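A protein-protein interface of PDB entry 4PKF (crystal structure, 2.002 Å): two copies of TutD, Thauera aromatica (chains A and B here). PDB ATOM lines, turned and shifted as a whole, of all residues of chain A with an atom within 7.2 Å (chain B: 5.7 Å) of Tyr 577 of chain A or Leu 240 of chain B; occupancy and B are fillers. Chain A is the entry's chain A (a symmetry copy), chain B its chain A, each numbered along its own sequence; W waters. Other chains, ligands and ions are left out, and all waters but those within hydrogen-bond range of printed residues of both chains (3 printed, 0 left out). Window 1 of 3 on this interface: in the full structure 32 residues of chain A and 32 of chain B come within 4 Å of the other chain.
Of the 19 printed residues of chain A, 7 touch a printed residue of chain B.
Printed residues of chain A that touch a printed residue of chain B: Tyr 172, Ser 570, Asp 573, Val 574, Tyr 577, Asn 695 and Tyr 696.
Hydrophobic or aromatic side chains of chain A within 4 Å of the printed part of chain B: Tyr 172, Val 574, Tyr 577 and Tyr 696.
Along chain A the printed residues that touch a printed residue of chain B span positions 172 to 696.
Printed residues of chain B that touch a printed residue of chain A: Trp 234, Gly 236, Thr 237, Leu 240 and Ile 243.
Hydrophobic or aromatic side chains of chain B within 4 Å of the printed part of chain A: Trp 234, Leu 240 and Ile 243.
Among the printed residues, 13 pairs touch across the chains.
NE1 of Trp 234 of chain B sits at hydrogen-bond distance from OD2 of Asp 573 of chain A, at 2.6 Å.
NH1 of Arg 581 of chain A is in hydrogen-bond range of O of Tyr 577 of chain A (2.9 Å).
The side-chain amide oxygen (OD1) of Asn 235 of chain B is in hydrogen-bond range of the side-chain hydroxyl (OG1) of Thr 237 of chain B (2.7 Å).
The side-chain hydroxyl of Tyr 696 of chain A is in hydrogen-bond range of the side-chain amide nitrogen of Gln 580 of chain A (3.3 Å).
OD1 of Asp 573 of chain A sits at hydrogen-bond distance from N of Tyr 696 of chain A (3.1 Å).
No position is printed for both chains.
Water W1 bridges the side-chain hydroxyl of Ser 570 of chain A (2.7 Å) and the backbone carbonyl oxygen of Met 229 of chain B (2.8 Å).
Water W2 lies within hydrogen-bond range of the side-chain hydroxyl of Tyr 577 of chain A (2.8 Å), the backbone carbonyl oxygen of Leu 240 of chain B (2.9 Å) and the backbone NH of Ala 244 of chain B (2.9 Å).
Water W3 lies within hydrogen-bond range of O of Tyr 172 of chain A (2.9 Å) and SD of Met 229 of chain B (3.1 Å).
Ile 243 of chain B touches Tyr 172 of chain A.
CB of Ser 570 of chain A touches CD2 of Trp 234 of chain B, at 3.5 Å.
Asp 573 of chain A touches Gly 236 of chain B.
Asp 573 of chain A touches Leu 240 of chain B.
Leu 240 of chain B touches Tyr 577 of chain A (O to CE2, 3.99 Å).
CD1 of Tyr 577 of chain A touches CD1 of Ile 243 of chain B (3.6 Å).
CA of Gly 236 of chain B touches C of Asn 695 of chain A (3.9 Å).
Asn 695 of chain A touches Thr 237 of chain B (O to CG2, 3.4 Å).
Tyr 696 of chain A touches Gly 236 of chain B.
O of Tyr 696 of chain A touches CG2 of Thr 237 of chain B, at 3.7 Å.
Of the printed residues of chain A, Leu 240 of chain B touches Asp 573, Val 574, Tyr 577 and Tyr 696.
No residue of chain A comes within 4 Å of Gly 239 of chain B.
Of the printed residues of chain B, Asn 695 of chain A touches Gly 236 and Thr 237.
Of the printed residues of chain B, Ser 570 of chain A touches Trp 234.
Of the printed residues of chain B, Val 574 of chain A touches Leu 240 (3.9 Å).
Printed residues of chain B within 4 Å of Tyr 696 of chain A: Gly 236, Thr 237 and Leu 240.
Asn 235 of chain B touches none of the printed residues of chain A.
Phe 578 of chain A touches none of the printed residues of chain B.
The nearest printed residue of chain B that does not touch Tyr 577 of chain A is Ala 244 of chain B (4.1 Å).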
ATOM      1  N   LEU A 165     -17.357  -4.938   9.412  1.00  0.00           N
ATOM      2  CA  LEU A 165     -16.836  -6.054  10.202  1.00  0.00           C
ATOM      3  C   LEU A 165     -17.777  -6.320  11.380  1.00  0.00           C
ATOM      4  O   LEU A 165     -18.072  -7.471  11.727  1.00  0.00           O
ATOM      5  CB  LEU A 165     -15.411  -5.757  10.684  1.00  0.00           C
ATOM      6  CG  LEU A 165     -14.706  -6.853  11.492  1.00  0.00           C
ATOM      7  CD1 LEU A 165     -14.543  -8.104  10.643  1.00  0.00           C
ATOM      8  CD2 LEU A 165     -13.348  -6.400  12.016  1.00  0.00           C
ATOM      9  N   CYS A 169     -19.727 -10.082  12.181  1.00  0.00           N
ATOM     10  CA  CYS A 169     -19.399 -10.911  13.334  1.00  0.00           C
ATOM     11  C   CYS A 169     -20.527 -11.102  14.340  1.00  0.00           C
ATOM     12  O   CYS A 169     -20.629 -12.149  14.967  1.00  0.00           O
ATOM     13  CB  CYS A 169     -18.209 -10.309  14.105  1.00  0.00           C
ATOM     14  SG  CYS A 169     -16.669 -10.281  13.189  1.00  0.00           S
ATOM     15  N   TYR A 172     -22.917 -14.409  15.204  1.00  0.00           N
ATOM     16  CA  TYR A 172     -22.448 -15.689  15.751  1.00  0.00           C
ATOM     17  C   TYR A 172     -22.423 -15.721  17.274  1.00  0.00           C
ATOM     18  O   TYR A 172     -21.866 -16.638  17.872  1.00  0.00           O
ATOM     19  CB  TYR A 172     -21.072 -16.025  15.167  1.00  0.00           C
ATOM     20  CG  TYR A 172     -21.264 -16.122  13.671  1.00  0.00           C
ATOM     21  CD1 TYR A 172     -21.881 -17.240  13.107  1.00  0.00           C
ATOM     22  CD2 TYR A 172     -20.936 -15.066  12.837  1.00  0.00           C
ATOM     23  CE1 TYR A 172     -22.125 -17.320  11.705  1.00  0.00           C
ATOM     24  CE2 TYR A 172     -21.191 -15.132  11.474  1.00  0.00           C
ATOM     25  CZ  TYR A 172     -21.769 -16.257  10.913  1.00  0.00           C
ATOM     26  OH  TYR A 172     -22.018 -16.279   9.553  1.00  0.00           O
ATOM     27  N   SER A 508      -6.693  -9.200  16.999  1.00  0.00           N
ATOM     28  CA  SER A 508      -7.443 -10.457  17.171  1.00  0.00           C
ATOM     29  C   SER A 508      -6.561 -11.613  17.646  1.00  0.00           C
ATOM     30  O   SER A 508      -7.063 -12.586  18.249  1.00  0.00           O
ATOM     31  CB  SER A 508      -8.134 -10.845  15.861  1.00  0.00           C
ATOM     32  OG  SER A 508      -9.037  -9.807  15.529  1.00  0.00           O
ATOM     33  N   SER A 570     -13.385 -15.919  22.070  1.00  0.00           N
ATOM     34  CA  SER A 570     -14.116 -16.410  20.910  1.00  0.00           C
ATOM     35  C   SER A 570     -14.499 -15.237  19.993  1.00  0.00           C
ATOM     36  O   SER A 570     -14.482 -15.383  18.773  1.00  0.00           O
ATOM     37  CB  SER A 570     -15.351 -17.253  21.320  1.00  0.00           C
ATOM     38  OG  SER A 570     -16.359 -16.517  21.986  1.00  0.00           O
ATOM     39  N   LYS A 572     -12.724 -12.536  19.503  1.00  0.00           N
ATOM     40  CA  LYS A 572     -11.507 -12.225  18.768  1.00  0.00           C
ATOM     41  C   LYS A 572     -11.251 -13.215  17.624  1.00  0.00           C
ATOM     42  O   LYS A 572     -10.850 -12.812  16.544  1.00  0.00           O
ATOM     43  CB  LYS A 572     -10.297 -12.202  19.718  1.00  0.00           C
ATOM     44  CG  LYS A 572     -10.245 -10.931  20.605  1.00  0.00           C
ATOM     45  CD  LYS A 572      -8.897 -10.767  21.319  1.00  0.00           C
ATOM     46  CE  LYS A 572      -8.588 -11.980  22.174  1.00  0.00           C
ATOM     47  NZ  LYS A 572      -7.416 -11.730  23.078  1.00  0.00           N
ATOM     48  N   ASP A 573     -11.465 -14.500  17.866  1.00  0.00           N
ATOM     49  CA  ASP A 573     -11.234 -15.491  16.808  1.00  0.00           C
ATOM     50  C   ASP A 573     -12.270 -15.389  15.699  1.00  0.00           C
ATOM     51  O   ASP A 573     -11.949 -15.619  14.546  1.00  0.00           O
ATOM     52  CB  ASP A 573     -11.203 -16.902  17.380  1.00  0.00           C
ATOM     53  CG  ASP A 573      -9.883 -17.221  18.098  1.00  0.00           C
ATOM     54  OD1 ASP A 573      -8.883 -16.491  17.920  1.00  0.00           O
ATOM     55  OD2 ASP A 573      -9.817 -18.235  18.832  1.00  0.00           O
ATOM     56  N   VAL A 574     -13.494 -14.989  16.010  1.00  0.00           N
ATOM     57  CA  VAL A 574     -14.478 -14.838  14.945  1.00  0.00           C
ATOM     58  C   VAL A 574     -14.087 -13.614  14.113  1.00  0.00           C
ATOM     59  O   VAL A 574     -14.179 -13.608  12.875  1.00  0.00           O
ATOM     60  CB  VAL A 574     -15.926 -14.713  15.515  1.00  0.00           C
ATOM     61  CG1 VAL A 574     -16.899 -14.205  14.457  1.00  0.00           C
ATOM     62  CG2 VAL A 574     -16.420 -16.082  16.055  1.00  0.00           C
ATOM     63  N   SER A 575     -13.619 -12.575  14.793  1.00  0.00           N
ATOM     64  CA  SER A 575     -13.189 -11.387  14.068  1.00  0.00           C
ATOM     65  C   SER A 575     -12.059 -11.766  13.095  1.00  0.00           C
ATOM     66  O   SER A 575     -12.062 -11.366  11.945  1.00  0.00           O
ATOM     67  CB  SER A 575     -12.725 -10.287  15.052  1.00  0.00           C
ATOM     68  OG  SER A 575     -12.265  -9.157  14.317  1.00  0.00           O
ATOM     69  N   ARG A 576     -11.114 -12.573  13.561  1.00  0.00           N
ATOM     70  CA  ARG A 576      -9.999 -13.059  12.726  1.00  0.00           C
ATOM     71  C   ARG A 576     -10.473 -13.762  11.451  1.00  0.00           C
ATOM     72  O   ARG A 576      -9.893 -13.607  10.361  1.00  0.00           O
ATOM     73  CB  ARG A 576      -9.132 -14.028  13.546  1.00  0.00           C
ATOM     74  CG  ARG A 576      -7.803 -14.477  12.887  1.00  0.00           C
ATOM     75  CD  ARG A 576      -6.799 -13.320  12.835  1.00  0.00           C
ATOM     76  NE  ARG A 576      -5.409 -13.758  12.616  1.00  0.00           N
ATOM     77  CZ  ARG A 576      -4.619 -14.196  13.593  1.00  0.00           C
ATOM     78  NH1 ARG A 576      -5.082 -14.252  14.845  1.00  0.00           N
ATOM     79  NH2 ARG A 576      -3.371 -14.539  13.329  1.00  0.00           N
ATOM     80  N   TYR A 577     -11.477 -14.616  11.632  1.00  0.00           N
ATOM     81  CA  TYR A 577     -12.088 -15.362  10.549  1.00  0.00           C
ATOM     82  C   TYR A 577     -12.582 -14.414   9.451  1.00  0.00           C
ATOM     83  O   TYR A 577     -12.338 -14.628   8.246  1.00  0.00           O
ATOM     84  CB  TYR A 577     -13.252 -16.214  11.113  1.00  0.00           C
ATOM     85  CG  TYR A 577     -13.927 -17.158  10.143  1.00  0.00           C
ATOM     86  CD1 TYR A 577     -14.980 -16.708   9.333  1.00  0.00           C
ATOM     87  CD2 TYR A 577     -13.554 -18.510  10.066  1.00  0.00           C
ATOM     88  CE1 TYR A 577     -15.639 -17.566   8.477  1.00  0.00           C
ATOM     89  CE2 TYR A 577     -14.220 -19.392   9.173  1.00  0.00           C
ATOM     90  CZ  TYR A 577     -15.264 -18.898   8.399  1.00  0.00           C
ATOM     91  OH  TYR A 577     -15.971 -19.702   7.531  1.00  0.00           O
ATOM     92  N   PHE A 578     -13.275 -13.353   9.850  1.00  0.00           N
ATOM     93  CA  PHE A 578     -13.781 -12.410   8.855  1.00  0.00           C
ATOM     94  C   PHE A 578     -12.772 -11.348   8.378  1.00  0.00           C
ATOM     95  O   PHE A 578     -12.860 -10.903   7.232  1.00  0.00           O
ATOM     96  CB  PHE A 578     -15.041 -11.755   9.384  1.00  0.00           C
ATOM     97  CG  PHE A 578     -16.211 -12.730   9.449  1.00  0.00           C
ATOM     98  CD1 PHE A 578     -16.787 -13.217   8.272  1.00  0.00           C
ATOM     99  CD2 PHE A 578     -16.664 -13.226  10.650  1.00  0.00           C
ATOM    100  CE1 PHE A 578     -17.847 -14.151   8.306  1.00  0.00           C
ATOM    101  CE2 PHE A 578     -17.745 -14.155  10.694  1.00  0.00           C
ATOM    102  CZ  PHE A 578     -18.326 -14.617   9.507  1.00  0.00           C
ATOM    103  N   GLU A 579     -11.833 -10.938   9.229  1.00  0.00           N
ATOM    104  CA  GLU A 579     -10.811  -9.987   8.782  1.00  0.00           C
ATOM    105  C   GLU A 579     -10.067 -10.526   7.556  1.00  0.00           C
ATOM    106  O   GLU A 579      -9.861  -9.818   6.578  1.00  0.00           O
ATOM    107  CB  GLU A 579      -9.791  -9.697   9.892  1.00  0.00           C
ATOM    108  CG  GLU A 579     -10.325  -8.901  11.036  1.00  0.00           C
ATOM    109  CD  GLU A 579      -9.387  -8.966  12.238  1.00  0.00           C
ATOM    110  OE1 GLU A 579      -9.768  -9.612  13.224  1.00  0.00           O
ATOM    111  OE2 GLU A 579      -8.271  -8.380  12.189  1.00  0.00           O
ATOM    112  N   GLN A 580      -9.667 -11.789   7.610  1.00  0.00           N
ATOM    113  CA  GLN A 580      -8.872 -12.350   6.523  1.00  0.00           C
ATOM    114  C   GLN A 580      -9.729 -12.607   5.287  1.00  0.00           C
ATOM    115  O   GLN A 580      -9.198 -12.785   4.195  1.00  0.00           O
ATOM    116  CB  GLN A 580      -8.229 -13.659   6.943  1.00  0.00           C
ATOM    117  CG  GLN A 580      -9.212 -14.848   7.019  1.00  0.00           C
ATOM    118  CD  GLN A 580      -8.548 -16.030   7.724  1.00  0.00           C
ATOM    119  OE1 GLN A 580      -8.094 -16.973   7.087  1.00  0.00           O
ATOM    120  NE2 GLN A 580      -8.449 -15.949   9.051  1.00  0.00           N
ATOM    121  N   ARG A 581     -11.044 -12.596   5.457  1.00  0.00           N
ATOM    122  CA  ARG A 581     -11.952 -12.855   4.343  1.00  0.00           C
ATOM    123  C   ARG A 581     -12.492 -11.581   3.697  1.00  0.00           C
ATOM    124  O   ARG A 581     -12.816 -11.586   2.512  1.00  0.00           O
ATOM    125  CB  ARG A 581     -13.122 -13.758   4.823  1.00  0.00           C
ATOM    126  CG  ARG A 581     -12.695 -15.212   4.964  1.00  0.00           C
ATOM    127  CD  ARG A 581     -13.778 -16.092   5.583  1.00  0.00           C
ATOM    128  NE  ARG A 581     -13.392 -17.497   5.549  1.00  0.00           N
ATOM    129  CZ  ARG A 581     -12.534 -18.055   6.390  1.00  0.00           C
ATOM    130  NH1 ARG A 581     -11.919 -17.327   7.325  1.00  0.00           N
ATOM    131  NH2 ARG A 581     -12.238 -19.334   6.274  1.00  0.00           N
ATOM    132  N   PHE A 582     -12.591 -10.494   4.453  1.00  0.00           N
ATOM    133  CA  PHE A 582     -13.211  -9.259   3.926  1.00  0.00           C
ATOM    134  C   PHE A 582     -12.429  -7.985   4.255  1.00  0.00           C
ATOM    135  O   PHE A 582     -12.696  -6.936   3.674  1.00  0.00           O
ATOM    136  CB  PHE A 582     -14.637  -9.107   4.461  1.00  0.00           C
ATOM    137  CG  PHE A 582     -15.543 -10.215   4.041  1.00  0.00           C
ATOM    138  CD1 PHE A 582     -16.108 -10.209   2.758  1.00  0.00           C
ATOM    139  CD2 PHE A 582     -15.784 -11.293   4.894  1.00  0.00           C
ATOM    140  CE1 PHE A 582     -16.933 -11.257   2.345  1.00  0.00           C
ATOM    141  CE2 PHE A 582     -16.614 -12.355   4.478  1.00  0.00           C
ATOM    142  CZ  PHE A 582     -17.190 -12.331   3.212  1.00  0.00           C
ATOM    143  N   CYS A 603      -3.754 -11.625   7.720  1.00  0.00           N
ATOM    144  CA  CYS A 603      -4.557 -12.133   8.843  1.00  0.00           C
ATOM    145  C   CYS A 603      -4.798 -13.622   8.799  1.00  0.00           C
ATOM    146  O   CYS A 603      -5.188 -14.208   9.803  1.00  0.00           O
ATOM    147  CB  CYS A 603      -5.897 -11.423   8.915  1.00  0.00           C
ATOM    148  SG  CYS A 603      -5.664  -9.783   9.644  1.00  0.00           S
ATOM    149  N   ASN A 695      -6.290 -20.219  20.969  1.00  0.00           N
ATOM    150  CA  ASN A 695      -6.823 -19.297  19.966  1.00  0.00           C
ATOM    151  C   ASN A 695      -6.648 -19.788  18.509  1.00  0.00           C
ATOM    152  O   ASN A 695      -6.279 -20.938  18.270  1.00  0.00           O
ATOM    153  CB  ASN A 695      -6.215 -17.894  20.176  1.00  0.00           C
ATOM    154  CG  ASN A 695      -4.768 -17.791  19.737  1.00  0.00           C
ATOM    155  OD1 ASN A 695      -4.073 -18.789  19.554  1.00  0.00           O
ATOM    156  ND2 ASN A 695      -4.301 -16.549  19.555  1.00  0.00           N
ATOM    157  N   TYR A 696      -6.999 -18.928  17.558  1.00  0.00           N
ATOM    158  CA  TYR A 696      -6.921 -19.212  16.139  1.00  0.00           C
ATOM    159  C   TYR A 696      -5.564 -19.802  15.723  1.00  0.00           C
ATOM    160  O   TYR A 696      -5.489 -20.671  14.884  1.00  0.00           O
ATOM    161  CB  TYR A 696      -7.167 -17.918  15.364  1.00  0.00           C
ATOM    162  CG  TYR A 696      -6.860 -17.988  13.886  1.00  0.00           C
ATOM    163  CD1 TYR A 696      -7.833 -18.425  12.979  1.00  0.00           C
ATOM    164  CD2 TYR A 696      -5.628 -17.564  13.380  1.00  0.00           C
ATOM    165  CE1 TYR A 696      -7.576 -18.480  11.577  1.00  0.00           C
ATOM    166  CE2 TYR A 696      -5.350 -17.619  11.970  1.00  0.00           C
ATOM    167  CZ  TYR A 696      -6.330 -18.082  11.080  1.00  0.00           C
ATOM    168  OH  TYR A 696      -6.116 -18.121   9.688  1.00  0.00           O
ATOM    169  N   MET B 229     -19.968 -23.506  20.488  1.00  0.00           N
ATOM    170  CA  MET B 229     -19.208 -22.274  20.405  1.00  0.00           C
ATOM    171  C   MET B 229     -19.205 -21.520  21.744  1.00  0.00           C
ATOM    172  O   MET B 229     -18.340 -20.682  22.002  1.00  0.00           O
ATOM    173  CB  MET B 229     -19.774 -21.414  19.278  1.00  0.00           C
ATOM    174  CG  MET B 229     -19.419 -21.949  17.839  1.00  0.00           C
ATOM    175  SD  MET B 229     -19.936 -20.737  16.622  1.00  0.00           S
ATOM    176  CE  MET B 229     -18.664 -19.463  16.844  1.00  0.00           C
ATOM    177  N   TRP B 234     -12.962 -22.471  25.062  1.00  0.00           N
ATOM    178  CA  TRP B 234     -12.924 -22.300  23.600  1.00  0.00           C
ATOM    179  C   TRP B 234     -11.600 -22.780  23.001  1.00  0.00           C
ATOM    180  O   TRP B 234     -10.521 -22.628  23.613  1.00  0.00           O
ATOM    181  CB  TRP B 234     -13.149 -20.810  23.270  1.00  0.00           C
ATOM    182  CG  TRP B 234     -12.850 -20.348  21.857  1.00  0.00           C
ATOM    183  CD1 TRP B 234     -11.686 -19.743  21.390  1.00  0.00           C
ATOM    184  CD2 TRP B 234     -13.765 -20.366  20.756  1.00  0.00           C
ATOM    185  NE1 TRP B 234     -11.828 -19.431  20.040  1.00  0.00           N
ATOM    186  CE2 TRP B 234     -13.094 -19.791  19.635  1.00  0.00           C
ATOM    187  CE3 TRP B 234     -15.090 -20.819  20.605  1.00  0.00           C
ATOM    188  CZ2 TRP B 234     -13.701 -19.668  18.393  1.00  0.00           C
ATOM    189  CZ3 TRP B 234     -15.696 -20.670  19.377  1.00  0.00           C
ATOM    190  CH2 TRP B 234     -14.993 -20.119  18.271  1.00  0.00           C
ATOM    191  N   ASN B 235     -11.696 -23.347  21.797  1.00  0.00           N
ATOM    192  CA  ASN B 235     -10.524 -23.705  21.007  1.00  0.00           C
ATOM    193  C   ASN B 235     -10.712 -23.135  19.618  1.00  0.00           C
ATOM    194  O   ASN B 235     -11.504 -23.667  18.820  1.00  0.00           O
ATOM    195  CB  ASN B 235     -10.332 -25.228  20.925  1.00  0.00           C
ATOM    196  CG  ASN B 235      -9.061 -25.608  20.185  1.00  0.00           C
ATOM    197  OD1 ASN B 235      -8.551 -24.851  19.337  1.00  0.00           O
ATOM    198  ND2 ASN B 235      -8.513 -26.767  20.524  1.00  0.00           N
ATOM    199  N   GLY B 236      -9.972 -22.071  19.316  1.00  0.00           N
ATOM    200  CA  GLY B 236     -10.147 -21.383  18.044  1.00  0.00           C
ATOM    201  C   GLY B 236      -9.712 -22.113  16.791  1.00  0.00           C
ATOM    202  O   GLY B 236     -10.036 -21.674  15.683  1.00  0.00           O
ATOM    203  N   THR B 237      -8.980 -23.212  16.943  1.00  0.00           N
ATOM    204  CA  THR B 237      -8.632 -24.044  15.783  1.00  0.00           C
ATOM    205  C   THR B 237      -9.749 -25.027  15.411  1.00  0.00           C
ATOM    206  O   THR B 237      -9.687 -25.691  14.377  1.00  0.00           O
ATOM    207  CB  THR B 237      -7.360 -24.819  16.035  1.00  0.00           C
ATOM    208  OG1 THR B 237      -7.598 -25.881  16.973  1.00  0.00           O
ATOM    209  CG2 THR B 237      -6.311 -23.889  16.575  1.00  0.00           C
ATOM    210  N   LYS B 238     -10.780 -25.102  16.255  1.00  0.00           N
ATOM    211  CA  LYS B 238     -11.923 -25.979  16.024  1.00  0.00           C
ATOM    212  C   LYS B 238     -13.231 -25.207  15.933  1.00  0.00           C
ATOM    213  O   LYS B 238     -14.073 -25.477  15.081  1.00  0.00           O
ATOM    214  CB  LYS B 238     -12.049 -27.012  17.154  1.00  0.00           C
ATOM    215  CG  LYS B 238     -10.850 -27.925  17.279  1.00  0.00           C
ATOM    216  CD  LYS B 238     -11.107 -29.003  18.327  1.00  0.00           C
ATOM    217  CE  LYS B 238      -9.949 -29.995  18.323  1.00  0.00           C
ATOM    218  NZ  LYS B 238     -10.195 -31.188  19.181  1.00  0.00           N
ATOM    219  N   GLY B 239     -13.414 -24.245  16.832  1.00  0.00           N
ATOM    220  CA  GLY B 239     -14.738 -23.686  17.034  1.00  0.00           C
ATOM    221  C   GLY B 239     -15.183 -22.842  15.851  1.00  0.00           C
ATOM    222  O   GLY B 239     -16.366 -22.609  15.654  1.00  0.00           O
ATOM    223  N   LEU B 240     -14.230 -22.348  15.078  1.00  0.00           N
ATOM    224  CA  LEU B 240     -14.571 -21.502  13.941  1.00  0.00           C
ATOM    225  C   LEU B 240     -15.174 -22.332  12.807  1.00  0.00           C
ATOM    226  O   LEU B 240     -15.834 -21.770  11.938  1.00  0.00           O
ATOM    227  CB  LEU B 240     -13.336 -20.747  13.426  1.00  0.00           C
ATOM    228  CG  LEU B 240     -12.722 -19.707  14.375  1.00  0.00           C
ATOM    229  CD1 LEU B 240     -11.522 -19.034  13.737  1.00  0.00           C
ATOM    230  CD2 LEU B 240     -13.800 -18.687  14.738  1.00  0.00           C
ATOM    231  N   ASP B 241     -14.939 -23.651  12.807  1.00  0.00           N
ATOM    232  CA  ASP B 241     -15.553 -24.526  11.785  1.00  0.00           C
ATOM    233  C   ASP B 241     -17.072 -24.437  11.849  1.00  0.00           C
ATOM    234  O   ASP B 241     -17.757 -24.747  10.890  1.00  0.00           O
ATOM    235  CB  ASP B 241     -15.139 -25.989  11.955  1.00  0.00           C
ATOM    236  CG  ASP B 241     -13.656 -26.201  11.755  1.00  0.00           C
ATOM    237  OD1 ASP B 241     -12.963 -25.238  11.363  1.00  0.00           O
ATOM    238  OD2 ASP B 241     -13.185 -27.332  11.994  1.00  0.00           O
ATOM    239  N   ASN B 242     -17.596 -24.006  12.987  1.00  0.00           N
ATOM    240  CA  ASN B 242     -19.050 -23.941  13.157  1.00  0.00           C
ATOM    241  C   ASN B 242     -19.680 -22.833  12.313  1.00  0.00           C
ATOM    242  O   ASN B 242     -20.877 -22.862  12.035  1.00  0.00           O
ATOM    243  CB  ASN B 242     -19.387 -23.730  14.650  1.00  0.00           C
ATOM    244  CG  ASN B 242     -19.154 -24.983  15.478  1.00  0.00           C
ATOM    245  OD1 ASN B 242     -19.657 -26.039  15.147  1.00  0.00           O
ATOM    246  ND2 ASN B 242     -18.307 -24.890  16.476  1.00  0.00           N
ATOM    247  N   ILE B 243     -18.888 -21.823  11.946  1.00  0.00           N
ATOM    248  CA  ILE B 243     -19.457 -20.691  11.216  1.00  0.00           C
ATOM    249  C   ILE B 243     -20.050 -21.142   9.855  1.00  0.00           C
ATOM    250  O   ILE B 243     -21.226 -20.899   9.566  1.00  0.00           O
ATOM    251  CB  ILE B 243     -18.408 -19.584  10.989  1.00  0.00           C
ATOM    252  CG1 ILE B 243     -18.072 -18.876  12.339  1.00  0.00           C
ATOM    253  CG2 ILE B 243     -18.910 -18.558   9.976  1.00  0.00           C
ATOM    254  CD1 ILE B 243     -16.834 -17.895  12.220  1.00  0.00           C
ATOM    255  N   ALA B 244     -19.237 -21.789   9.040  1.00  0.00           N
ATOM    256  CA  ALA B 244     -19.714 -22.225   7.726  1.00  0.00           C
ATOM    257  C   ALA B 244     -20.828 -23.264   7.868  1.00  0.00           C
ATOM    258  O   ALA B 244     -21.769 -23.249   7.074  1.00  0.00           O
ATOM    259  CB  ALA B 244     -18.582 -22.765   6.880  1.00  0.00           C
HETATM  260  O   HOH W   1     -18.637 -17.936  22.061  1.00  0.00           O
HETATM  261  O   HOH W   2     -16.374 -21.958   9.139  1.00  0.00           O
HETATM  262  O   HOH W   3     -22.663 -19.206  16.710  1.00  0.00           O
